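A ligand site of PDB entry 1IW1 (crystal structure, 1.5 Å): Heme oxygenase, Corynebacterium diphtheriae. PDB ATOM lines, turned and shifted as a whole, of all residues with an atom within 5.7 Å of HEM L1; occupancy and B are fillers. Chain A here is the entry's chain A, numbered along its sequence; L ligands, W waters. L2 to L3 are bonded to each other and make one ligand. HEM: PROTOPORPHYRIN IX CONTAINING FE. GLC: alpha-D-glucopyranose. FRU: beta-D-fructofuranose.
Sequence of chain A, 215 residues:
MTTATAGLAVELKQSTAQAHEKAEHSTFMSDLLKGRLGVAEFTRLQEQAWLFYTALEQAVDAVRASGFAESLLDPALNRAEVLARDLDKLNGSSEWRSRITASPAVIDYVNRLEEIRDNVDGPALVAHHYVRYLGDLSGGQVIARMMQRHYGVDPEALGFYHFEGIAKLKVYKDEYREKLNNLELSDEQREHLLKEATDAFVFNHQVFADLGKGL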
ATOM      1  N   ALA A   9       1.091  30.292 -16.620  1.00  0.00           N
ATOM      2  CA  ALA A   9      -0.179  30.291 -15.893  1.00  0.00           C
ATOM      3  C   ALA A   9      -1.350  30.096 -16.857  1.00  0.00           C
ATOM      4  O   ALA A   9      -2.240  29.292 -16.637  1.00  0.00           O
ATOM      5  CB  ALA A   9      -0.329  31.546 -15.081  1.00  0.00           C
ATOM      6  N   LEU A  12      -1.214  26.560 -18.530  1.00  0.00           N
ATOM      7  CA  LEU A  12      -1.744  25.567 -17.582  1.00  0.00           C
ATOM      8  C   LEU A  12      -3.228  25.547 -17.546  1.00  0.00           C
ATOM      9  O   LEU A  12      -3.855  24.487 -17.616  1.00  0.00           O
ATOM     10  CB  LEU A  12      -1.289  25.874 -16.148  1.00  0.00           C
ATOM     11  CG  LEU A  12      -0.127  25.083 -15.642  1.00  0.00           C
ATOM     12  CD1 LEU A  12       0.288  25.662 -14.304  1.00  0.00           C
ATOM     13  CD2 LEU A  12      -0.339  23.555 -15.561  1.00  0.00           C
ATOM     14  N   LYS A  13      -3.809  26.738 -17.412  1.00  0.00           N
ATOM     15  CA  LYS A  13      -5.259  26.876 -17.353  1.00  0.00           C
ATOM     16  C   LYS A  13      -5.908  26.284 -18.614  1.00  0.00           C
ATOM     17  O   LYS A  13      -6.859  25.502 -18.533  1.00  0.00           O
ATOM     18  CB  LYS A  13      -5.617  28.337 -17.153  1.00  0.00           C
ATOM     19  CG  LYS A  13      -7.066  28.589 -16.835  1.00  0.00           C
ATOM     20  CD  LYS A  13      -7.247  30.060 -16.538  1.00  0.00           C
ATOM     21  CE  LYS A  13      -8.567  30.350 -15.932  1.00  0.00           C
ATOM     22  NZ  LYS A  13      -9.516  30.248 -16.997  1.00  0.00           N
ATOM     23  N   HIS A  20     -10.229  19.675 -16.008  1.00  0.00           N
ATOM     24  CA  HIS A  20     -10.909  20.364 -14.907  1.00  0.00           C
ATOM     25  C   HIS A  20     -12.419  20.196 -15.001  1.00  0.00           C
ATOM     26  O   HIS A  20     -13.079  19.835 -14.016  1.00  0.00           O
ATOM     27  CB  HIS A  20     -10.517  21.851 -14.883  1.00  0.00           C
ATOM     28  CG  HIS A  20     -11.273  22.655 -13.878  1.00  0.00           C
ATOM     29  ND1 HIS A  20     -12.489  23.235 -14.158  1.00  0.00           N
ATOM     30  CD2 HIS A  20     -11.008  22.950 -12.582  1.00  0.00           C
ATOM     31  CE1 HIS A  20     -12.928  23.883 -13.099  1.00  0.00           C
ATOM     32  NE2 HIS A  20     -12.079  23.679 -12.101  1.00  0.00           N
ATOM     33  N   ALA A  23     -13.407  16.691 -13.866  1.00  0.00           N
ATOM     34  CA  ALA A  23     -13.333  16.507 -12.423  1.00  0.00           C
ATOM     35  C   ALA A  23     -14.484  17.238 -11.735  1.00  0.00           C
ATOM     36  O   ALA A  23     -15.153  16.656 -10.893  1.00  0.00           O
ATOM     37  CB  ALA A  23     -11.987  17.007 -11.915  1.00  0.00           C
ATOM     38  N   GLU A  24     -14.646  18.517 -12.057  1.00  0.00           N
ATOM     39  CA  GLU A  24     -15.682  19.377 -11.471  1.00  0.00           C
ATOM     40  C   GLU A  24     -17.063  18.808 -11.600  1.00  0.00           C
ATOM     41  O   GLU A  24     -17.877  18.940 -10.688  1.00  0.00           O
ATOM     42  CB  GLU A  24     -15.608  20.771 -12.146  1.00  0.00           C
ATOM     43  CG  GLU A  24     -16.835  21.655 -12.170  1.00  0.00           C
ATOM     44  CD  GLU A  24     -16.519  22.981 -12.840  1.00  0.00           C
ATOM     45  OE1 GLU A  24     -15.860  22.995 -13.941  1.00  0.00           O
ATOM     46  OE2 GLU A  24     -16.894  24.009 -12.290  1.00  0.00           O
ATOM     47  N   MET A  29     -19.310  14.707  -7.077  1.00  0.00           N
ATOM     48  CA  MET A  29     -19.212  16.095  -6.690  1.00  0.00           C
ATOM     49  C   MET A  29     -20.465  16.860  -7.070  1.00  0.00           C
ATOM     50  O   MET A  29     -20.916  17.717  -6.321  1.00  0.00           O
ATOM     51  CB  MET A  29     -17.960  16.745  -7.287  1.00  0.00           C
ATOM     52  CG  MET A  29     -17.712  18.225  -6.897  1.00  0.00           C
ATOM     53  SD  MET A  29     -17.790  18.596  -5.113  1.00  0.00           S
ATOM     54  CE  MET A  29     -16.488  17.648  -4.555  1.00  0.00           C
ATOM     55  N   LEU A  33     -22.712  18.840  -4.273  1.00  0.00           N
ATOM     56  CA  LEU A  33     -22.936  20.275  -4.277  1.00  0.00           C
ATOM     57  C   LEU A  33     -24.377  20.691  -4.458  1.00  0.00           C
ATOM     58  O   LEU A  33     -24.742  21.788  -4.023  1.00  0.00           O
ATOM     59  CB  LEU A  33     -22.062  20.941  -5.335  1.00  0.00           C
ATOM     60  CG  LEU A  33     -20.573  20.803  -5.046  1.00  0.00           C
ATOM     61  CD1 LEU A  33     -19.787  21.517  -6.134  1.00  0.00           C
ATOM     62  CD2 LEU A  33     -20.226  21.295  -3.680  1.00  0.00           C
ATOM     63  N   TYR A 130      -0.405  23.302  -7.976  1.00  0.00           N
ATOM     64  CA  TYR A 130      -1.330  24.179  -8.681  1.00  0.00           C
ATOM     65  C   TYR A 130      -2.725  23.569  -8.720  1.00  0.00           C
ATOM     66  O   TYR A 130      -3.727  24.217  -8.339  1.00  0.00           O
ATOM     67  CB  TYR A 130      -0.820  24.388 -10.116  1.00  0.00           C
ATOM     68  CG  TYR A 130      -1.870  24.850 -11.115  1.00  0.00           C
ATOM     69  CD1 TYR A 130      -2.285  26.162 -11.171  1.00  0.00           C
ATOM     70  CD2 TYR A 130      -2.431  23.935 -12.006  1.00  0.00           C
ATOM     71  CE1 TYR A 130      -3.230  26.586 -12.097  1.00  0.00           C
ATOM     72  CE2 TYR A 130      -3.379  24.324 -12.921  1.00  0.00           C
ATOM     73  CZ  TYR A 130      -3.790  25.657 -12.946  1.00  0.00           C
ATOM     74  OH  TYR A 130      -4.762  26.076 -13.862  1.00  0.00           O
ATOM     75  N   VAL A 131      -2.837  22.325  -9.130  1.00  0.00           N
ATOM     76  CA  VAL A 131      -4.139  21.678  -9.296  1.00  0.00           C
ATOM     77  C   VAL A 131      -4.897  21.641  -7.966  1.00  0.00           C
ATOM     78  O   VAL A 131      -6.072  22.015  -7.897  1.00  0.00           O
ATOM     79  CB  VAL A 131      -3.978  20.291  -9.946  1.00  0.00           C
ATOM     80  CG1 VAL A 131      -5.273  19.478  -9.940  1.00  0.00           C
ATOM     81  CG2 VAL A 131      -3.553  20.484 -11.363  1.00  0.00           C
ATOM     82  N   ARG A 132      -4.240  21.239  -6.885  1.00  0.00           N
ATOM     83  CA  ARG A 132      -4.955  21.162  -5.625  1.00  0.00           C
ATOM     84  C   ARG A 132      -5.187  22.514  -4.990  1.00  0.00           C
ATOM     85  O   ARG A 132      -6.343  22.857  -4.683  1.00  0.00           O
ATOM     86  CB  ARG A 132      -4.260  20.229  -4.633  1.00  0.00           C
ATOM     87  CG  ARG A 132      -4.539  18.730  -4.841  1.00  0.00           C
ATOM     88  CD  ARG A 132      -6.011  18.321  -5.044  1.00  0.00           C
ATOM     89  NE  ARG A 132      -6.876  18.885  -4.038  1.00  0.00           N
ATOM     90  CZ  ARG A 132      -8.165  18.633  -3.881  1.00  0.00           C
ATOM     91  NH1 ARG A 132      -8.762  17.715  -4.622  1.00  0.00           N
ATOM     92  NH2 ARG A 132      -8.878  19.313  -2.964  1.00  0.00           N
ATOM     93  N   LEU A 134      -4.794  25.780  -5.977  1.00  0.00           N
ATOM     94  CA  LEU A 134      -5.576  26.813  -6.669  1.00  0.00           C
ATOM     95  C   LEU A 134      -7.049  26.390  -6.759  1.00  0.00           C
ATOM     96  O   LEU A 134      -7.972  27.247  -6.709  1.00  0.00           O
ATOM     97  CB  LEU A 134      -4.982  27.181  -8.018  1.00  0.00           C
ATOM     98  CG  LEU A 134      -4.992  28.659  -8.338  1.00  0.00           C
ATOM     99  CD1 LEU A 134      -4.623  29.519  -7.260  1.00  0.00           C
ATOM    100  CD2 LEU A 134      -4.168  29.000  -9.559  1.00  0.00           C
ATOM    101  N   GLY A 135      -7.294  25.083  -6.825  1.00  0.00           N
ATOM    102  CA  GLY A 135      -8.646  24.550  -6.795  1.00  0.00           C
ATOM    103  C   GLY A 135      -9.304  24.868  -5.464  1.00  0.00           C
ATOM    104  O   GLY A 135     -10.460  25.314  -5.410  1.00  0.00           O
ATOM    105  N   ASP A 136      -8.579  24.674  -4.359  1.00  0.00           N
ATOM    106  CA  ASP A 136      -9.112  24.954  -3.016  1.00  0.00           C
ATOM    107  C   ASP A 136      -9.458  26.407  -2.819  1.00  0.00           C
ATOM    108  O   ASP A 136     -10.458  26.744  -2.133  1.00  0.00           O
ATOM    109  CB  ASP A 136      -8.108  24.558  -1.922  1.00  0.00           C
ATOM    110  CG  ASP A 136      -7.725  23.101  -1.953  1.00  0.00           C
ATOM    111  OD1 ASP A 136      -6.589  22.788  -1.488  1.00  0.00           O
ATOM    112  OD2 ASP A 136      -8.521  22.225  -2.376  1.00  0.00           O
ATOM    113  N   LEU A 137      -8.624  27.257  -3.400  1.00  0.00           N
ATOM    114  CA  LEU A 137      -8.782  28.706  -3.347  1.00  0.00           C
ATOM    115  C   LEU A 137      -9.839  29.197  -4.349  1.00  0.00           C
ATOM    116  O   LEU A 137     -10.176  30.407  -4.372  1.00  0.00           O
ATOM    117  CB  LEU A 137      -7.458  29.374  -3.658  1.00  0.00           C
ATOM    118  CG  LEU A 137      -6.365  29.173  -2.632  1.00  0.00           C
ATOM    119  CD1 LEU A 137      -5.029  29.705  -3.164  1.00  0.00           C
ATOM    120  CD2 LEU A 137      -6.708  29.796  -1.281  1.00  0.00           C
ATOM    121  N   SER A 138     -10.404  28.281  -5.109  1.00  0.00           N
ATOM    122  CA  SER A 138     -11.376  28.630  -6.156  1.00  0.00           C
ATOM    123  C   SER A 138     -12.672  27.849  -5.921  1.00  0.00           C
ATOM    124  O   SER A 138     -13.506  28.288  -5.117  1.00  0.00           O
ATOM    125  CB  SER A 138     -10.739  28.365  -7.542  1.00  0.00           C
ATOM    126  OG  SER A 138      -9.579  29.152  -7.711  1.00  0.00           O
ATOM    127  N   GLY A 139     -12.835  26.706  -6.577  1.00  0.00           N
ATOM    128  CA  GLY A 139     -13.983  25.825  -6.379  1.00  0.00           C
ATOM    129  C   GLY A 139     -14.224  25.444  -4.934  1.00  0.00           C
ATOM    130  O   GLY A 139     -15.353  25.245  -4.477  1.00  0.00           O
ATOM    131  N   GLY A 140     -13.128  25.286  -4.199  1.00  0.00           N
ATOM    132  CA  GLY A 140     -13.236  24.948  -2.791  1.00  0.00           C
ATOM    133  C   GLY A 140     -14.132  25.877  -1.994  1.00  0.00           C
ATOM    134  O   GLY A 140     -14.847  25.469  -1.072  1.00  0.00           O
ATOM    135  N   VAL A 142     -16.745  27.403  -3.006  1.00  0.00           N
ATOM    136  CA  VAL A 142     -18.146  27.069  -3.304  1.00  0.00           C
ATOM    137  C   VAL A 142     -18.509  25.808  -2.503  1.00  0.00           C
ATOM    138  O   VAL A 142     -19.616  25.701  -1.958  1.00  0.00           O
ATOM    139  CB  VAL A 142     -18.363  26.806  -4.812  1.00  0.00           C
ATOM    140  CG1 VAL A 142     -19.797  26.350  -5.120  1.00  0.00           C
ATOM    141  CG2 VAL A 142     -17.970  28.022  -5.580  1.00  0.00           C
ATOM    142  N   ILE A 143     -17.606  24.818  -2.480  1.00  0.00           N
ATOM    143  CA  ILE A 143     -17.854  23.612  -1.717  1.00  0.00           C
ATOM    144  C   ILE A 143     -18.149  23.946  -0.259  1.00  0.00           C
ATOM    145  O   ILE A 143     -19.122  23.445   0.286  1.00  0.00           O
ATOM    146  CB  ILE A 143     -16.649  22.577  -1.833  1.00  0.00           C
ATOM    147  CG1 ILE A 143     -16.460  22.158  -3.271  1.00  0.00           C
ATOM    148  CG2 ILE A 143     -16.884  21.372  -0.943  1.00  0.00           C
ATOM    149  CD1 ILE A 143     -15.176  21.362  -3.512  1.00  0.00           C
ATOM    150  N   LYS A 173      -3.993  34.549  -5.438  1.00  0.00           N
ATOM    151  CA  LYS A 173      -3.965  33.774  -6.660  1.00  0.00           C
ATOM    152  C   LYS A 173      -3.262  34.485  -7.794  1.00  0.00           C
ATOM    153  O   LYS A 173      -2.596  33.859  -8.625  1.00  0.00           O
ATOM    154  CB  LYS A 173      -5.382  33.358  -7.118  1.00  0.00           C
ATOM    155  CG  LYS A 173      -5.991  32.288  -6.247  1.00  0.00           C
ATOM    156  CD  LYS A 173      -7.193  31.634  -6.919  1.00  0.00           C
ATOM    157  CE  LYS A 173      -8.384  32.502  -6.820  1.00  0.00           C
ATOM    158  NZ  LYS A 173      -9.628  31.901  -7.450  1.00  0.00           N
ATOM    159  N   ARG A 177       0.020  33.027  -9.773  1.00  0.00           N
ATOM    160  CA  ARG A 177       0.206  32.913 -11.215  1.00  0.00           C
ATOM    161  C   ARG A 177       1.459  33.669 -11.706  1.00  0.00           C
ATOM    162  O   ARG A 177       2.151  33.209 -12.606  1.00  0.00           O
ATOM    163  CB  ARG A 177      -1.024  33.406 -11.966  1.00  0.00           C
ATOM    164  CG  ARG A 177      -2.247  32.634 -11.706  1.00  0.00           C
ATOM    165  CD  ARG A 177      -3.378  32.992 -12.641  1.00  0.00           C
ATOM    166  NE  ARG A 177      -4.580  32.335 -12.217  1.00  0.00           N
ATOM    167  CZ  ARG A 177      -5.477  32.839 -11.352  1.00  0.00           C
ATOM    168  NH1 ARG A 177      -5.336  34.038 -10.837  1.00  0.00           N
ATOM    169  NH2 ARG A 177      -6.512  32.107 -11.000  1.00  0.00           N
ATOM    170  N   PHE A 201      -5.422  16.158 -12.465  1.00  0.00           N
ATOM    171  CA  PHE A 201      -6.859  16.255 -12.564  1.00  0.00           C
ATOM    172  C   PHE A 201      -7.481  14.881 -12.783  1.00  0.00           C
ATOM    173  O   PHE A 201      -8.554  14.583 -12.283  1.00  0.00           O
ATOM    174  CB  PHE A 201      -7.270  17.156 -13.734  1.00  0.00           C
ATOM    175  CG  PHE A 201      -7.358  18.611 -13.367  1.00  0.00           C
ATOM    176  CD1 PHE A 201      -6.448  19.527 -13.785  1.00  0.00           C
ATOM    177  CD2 PHE A 201      -8.368  19.060 -12.535  1.00  0.00           C
ATOM    178  CE1 PHE A 201      -6.553  20.872 -13.437  1.00  0.00           C
ATOM    179  CE2 PHE A 201      -8.507  20.380 -12.221  1.00  0.00           C
ATOM    180  CZ  PHE A 201      -7.601  21.286 -12.625  1.00  0.00           C
ATOM    181  N   ASN A 204      -7.772  13.135  -9.553  1.00  0.00           N
ATOM    182  CA  ASN A 204      -8.874  13.721  -8.761  1.00  0.00           C
ATOM    183  C   ASN A 204     -10.259  13.272  -9.250  1.00  0.00           C
ATOM    184  O   ASN A 204     -11.154  13.038  -8.444  1.00  0.00           O
ATOM    185  CB  ASN A 204      -8.732  15.231  -8.682  1.00  0.00           C
ATOM    186  CG  ASN A 204      -7.788  15.650  -7.590  1.00  0.00           C
ATOM    187  OD1 ASN A 204      -8.138  15.641  -6.413  1.00  0.00           O
ATOM    188  ND2 ASN A 204      -6.527  15.974  -7.957  1.00  0.00           N
ATOM    189  N   PHE A 208     -13.196  10.934  -7.083  1.00  0.00           N
ATOM    190  CA  PHE A 208     -14.633  11.159  -7.001  1.00  0.00           C
ATOM    191  C   PHE A 208     -15.400   9.952  -7.494  1.00  0.00           C
ATOM    192  O   PHE A 208     -16.409   9.570  -6.891  1.00  0.00           O
ATOM    193  CB  PHE A 208     -15.035  12.361  -7.816  1.00  0.00           C
ATOM    194  CG  PHE A 208     -14.561  13.695  -7.305  1.00  0.00           C
ATOM    195  CD1 PHE A 208     -14.548  14.028  -5.974  1.00  0.00           C
ATOM    196  CD2 PHE A 208     -14.223  14.673  -8.212  1.00  0.00           C
ATOM    197  CE1 PHE A 208     -14.171  15.297  -5.543  1.00  0.00           C
ATOM    198  CE2 PHE A 208     -13.819  15.937  -7.800  1.00  0.00           C
ATOM    199  CZ  PHE A 208     -13.798  16.252  -6.458  1.00  0.00           C
HETATM  200  CHA HEM L   1     -10.646  27.365 -10.764  1.00  0.00           C
HETATM  201  CHB HEM L   1      -9.010  22.945  -9.636  1.00  0.00           C
HETATM  202  CHC HEM L   1     -13.411  21.523  -8.614  1.00  0.00           C
HETATM  203  CHD HEM L   1     -15.153  25.827  -9.928  1.00  0.00           C
HETATM  204  C1A HEM L   1      -9.736  26.257 -10.562  1.00  0.00           C
HETATM  205  C2A HEM L   1      -8.342  26.403 -10.778  1.00  0.00           C
HETATM  206  C3A HEM L   1      -7.876  25.121 -10.452  1.00  0.00           C
HETATM  207  C4A HEM L   1      -8.950  24.258 -10.074  1.00  0.00           C
HETATM  208  CMA HEM L   1      -6.467  24.564 -10.515  1.00  0.00           C
HETATM  209  CAA HEM L   1      -7.509  27.541 -11.234  1.00  0.00           C
HETATM  210  CBA HEM L   1      -7.576  27.804 -12.690  1.00  0.00           C
HETATM  211  CGA HEM L   1      -6.591  28.862 -13.079  1.00  0.00           C
HETATM  212  O1A HEM L   1      -6.876  30.090 -12.863  1.00  0.00           O
HETATM  213  O2A HEM L   1      -5.492  28.563 -13.639  1.00  0.00           O
HETATM  214  C1B HEM L   1      -9.950  22.111  -9.254  1.00  0.00           C
HETATM  215  C2B HEM L   1      -9.950  20.757  -8.815  1.00  0.00           C
HETATM  216  C3B HEM L   1     -11.115  20.333  -8.526  1.00  0.00           C
HETATM  217  C4B HEM L   1     -12.024  21.504  -8.835  1.00  0.00           C
HETATM  218  CMB HEM L   1      -8.661  20.023  -8.703  1.00  0.00           C
HETATM  219  CAB HEM L   1     -11.630  19.039  -8.052  1.00  0.00           C
HETATM  220  CBB HEM L   1     -10.800  18.140  -7.285  1.00  0.00           C
HETATM  221  C1C HEM L   1     -14.282  22.569  -8.844  1.00  0.00           C
HETATM  222  C2C HEM L   1     -15.653  22.537  -8.487  1.00  0.00           C
HETATM  223  C3C HEM L   1     -16.160  23.704  -8.951  1.00  0.00           C
HETATM  224  C4C HEM L   1     -15.138  24.558  -9.452  1.00  0.00           C
HETATM  225  CMC HEM L   1     -16.453  21.363  -7.975  1.00  0.00           C
HETATM  226  CAC HEM L   1     -17.639  24.153  -8.877  1.00  0.00           C
HETATM  227  CBC HEM L   1     -17.904  24.654  -7.654  1.00  0.00           C
HETATM  228  C1D HEM L   1     -14.135  26.642 -10.259  1.00  0.00           C
HETATM  229  C2D HEM L   1     -14.106  27.999 -10.658  1.00  0.00           C
HETATM  230  C3D HEM L   1     -12.839  28.486 -10.912  1.00  0.00           C
HETATM  231  C4D HEM L   1     -12.010  27.309 -10.599  1.00  0.00           C
HETATM  232  CMD HEM L   1     -15.424  28.779 -10.804  1.00  0.00           C
HETATM  233  CAD HEM L   1     -12.448  29.804 -11.357  1.00  0.00           C
HETATM  234  CBD HEM L   1     -11.882  30.686 -10.248  1.00  0.00           C
HETATM  235  CGD HEM L   1     -12.830  31.051  -9.205  1.00  0.00           C
HETATM  236  O1D HEM L   1     -13.991  31.414  -9.558  1.00  0.00           O
HETATM  237  O2D HEM L   1     -12.616  31.068  -7.960  1.00  0.00           O
HETATM  238  NA  HEM L   1     -10.143  25.035 -10.124  1.00  0.00           N
HETATM  239  NB  HEM L   1     -11.291  22.527  -9.234  1.00  0.00           N
HETATM  240  NC  HEM L   1     -13.929  23.757  -9.372  1.00  0.00           N
HETATM  241  ND  HEM L   1     -12.790  26.247 -10.249  1.00  0.00           N
HETATM  242 FE   HEM L   1     -12.084  24.332 -10.005  1.00  0.00          FE
HETATM  243  C1  GLC L   2     -15.313  26.841 -18.094  1.00  0.00           C
HETATM  244  C2  GLC L   2     -15.915  27.343 -19.408  1.00  0.00           C
HETATM  245  C3  GLC L   2     -15.624  28.820 -19.594  1.00  0.00           C
HETATM  246  C4  GLC L   2     -16.213  29.579 -18.418  1.00  0.00           C
HETATM  247  C5  GLC L   2     -15.618  29.008 -17.119  1.00  0.00           C
HETATM  248  C6  GLC L   2     -16.301  29.624 -15.897  1.00  0.00           C
HETATM  249  O2  GLC L   2     -15.373  26.540 -20.438  1.00  0.00           O
HETATM  250  O3  GLC L   2     -16.191  29.321 -20.827  1.00  0.00           O
HETATM  251  O4  GLC L   2     -15.904  30.944 -18.542  1.00  0.00           O
HETATM  252  O5  GLC L   2     -15.839  27.607 -17.006  1.00  0.00           O
HETATM  253  O6  GLC L   2     -15.758  29.163 -14.655  1.00  0.00           O
HETATM  254  C1  FRU L   3     -13.410  24.560 -17.885  1.00  0.00           C
HETATM  255  C2  FRU L   3     -13.114  25.982 -17.459  1.00  0.00           C
HETATM  256  C3  FRU L   3     -11.650  26.393 -17.622  1.00  0.00           C
HETATM  257  C4  FRU L   3     -11.415  27.317 -16.450  1.00  0.00           C
HETATM  258  C5  FRU L   3     -12.206  26.571 -15.401  1.00  0.00           C
HETATM  259  C6  FRU L   3     -12.600  27.414 -14.194  1.00  0.00           C
HETATM  260  O1  FRU L   3     -12.657  23.676 -17.047  1.00  0.00           O
HETATM  261  O2  FRU L   3     -13.895  26.943 -18.196  1.00  0.00           O
HETATM  262  O3  FRU L   3     -11.380  27.003 -18.904  1.00  0.00           O
HETATM  263  O4  FRU L   3     -10.050  27.553 -16.102  1.00  0.00           O
HETATM  264  O5  FRU L   3     -13.393  26.088 -16.054  1.00  0.00           O
HETATM  265  O6  FRU L   3     -13.134  28.694 -14.582  1.00  0.00           O
HETATM  266  O   HOH W   1      -8.510  21.451  -5.593  1.00  0.00           O
HETATM  267  O   HOH W   2     -11.906  32.187  -4.773  1.00  0.00           O
HETATM  268  O   HOH W   3     -14.223  30.994  -5.784  1.00  0.00           O
HETATM  269  O   HOH W   4      -6.924  32.467 -14.165  1.00  0.00           O
HETATM  270  O   HOH W   5     -11.283  21.497  -5.466  1.00  0.00           O
HETATM  271  O   HOH W   6      -9.423  30.806 -12.295  1.00  0.00           O
HETATM  272  O   HOH W   7      -3.794  30.286 -14.563  1.00  0.00           O
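A ring nitrogen (ND1) of His 20 lies close to the side-chain carboxylate of Glu 24, 3.4 Å away.
NZ of Lys 173 is in hydrogen-bond range of OG of Ser 138, at 2.8 Å.
The side-chain amino group (NZ) of Lys 173 is in hydrogen-bond range of the backbone carbonyl oxygen (O) of Leu 137.
The side-chain hydroxyl (OG) of Ser 138 sits at hydrogen-bond distance from the backbone carbonyl oxygen (O) of Leu 134 (2.7 Å).
The backbone carbonyl oxygen (O) of Gly 135 sits at hydrogen-bond distance from the backbone NH (N) of Gly 140 (2.9 Å).
The guanidinium group (NH1) of Arg 132 is in hydrogen-bond range of the side-chain amide oxygen (OD1) of Asn 204, at 2.8 Å.
NH2 of Arg 132 is in salt-bridge range of OD2 of Asp 136 (3.0 Å).
NE2 of His 20 binds FE of HEM L1.
O2A of HEM L1 is in hydrogen-bond range of OH of Tyr 130, at 2.6 Å.
The guanidinium group (NH2) of Arg 177 lies within salt-bridge range of an oxygen (O1A) of HEM L1 (2.8 Å).
NZ of Lys 173 is in salt-bridge range of O2D of HEM L1, 3.1 Å away.
A ring nitrogen (ND1) of His 20 sits at hydrogen-bond distance from an oxygen (O1) of FRU L3 (2.9 Å).
O4 of FRU L3 lies within hydrogen-bond range of NZ of Lys 13, 2.9 Å away.
Water W7 lies within hydrogen-bond range of an oxygen (O2A) of HEM L1 (2.6 Å), the backbone carbonyl oxygen of Ala 9 (2.8 Å) and the guanidinium group of Arg 177 (3.2 Å).
Water W3 bridges an oxygen (O2D) of HEM L1 (2.7 Å) and the backbone carbonyl oxygen of Ser 138 (2.9 Å).
Water W6 bridges O1A of HEM L1 and NH2 of Arg 177.
Water W4 bridges an oxygen (O1A) of HEM L1 (2.7 Å) and the guanidinium group (NE) of Arg 177 (3.1 Å).
Water W2 bridges the backbone carbonyl oxygen (O) of Leu 137 (2.5 Å) and an oxygen (O2D) of HEM L1 (3.5 Å).
Residues that only touch HEM L1: Lys 13, Glu 24, Met 29, Leu 33, Val 131, Arg 132, Leu 134, Gly 135, Ser 138, Gly 139, Val 142, Phe 201, Asn 204 and Phe 208.
Hydrophobic or aromatic side chains within 4 Å of HEM L1: His 20, Met 29, Leu 33, Tyr 130, Val 131, Leu 134, Val 142, Phe 201 and Phe 208.
The nearest printed residue that does not touch HEM L1 is Ala 23 (4.4 Å).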
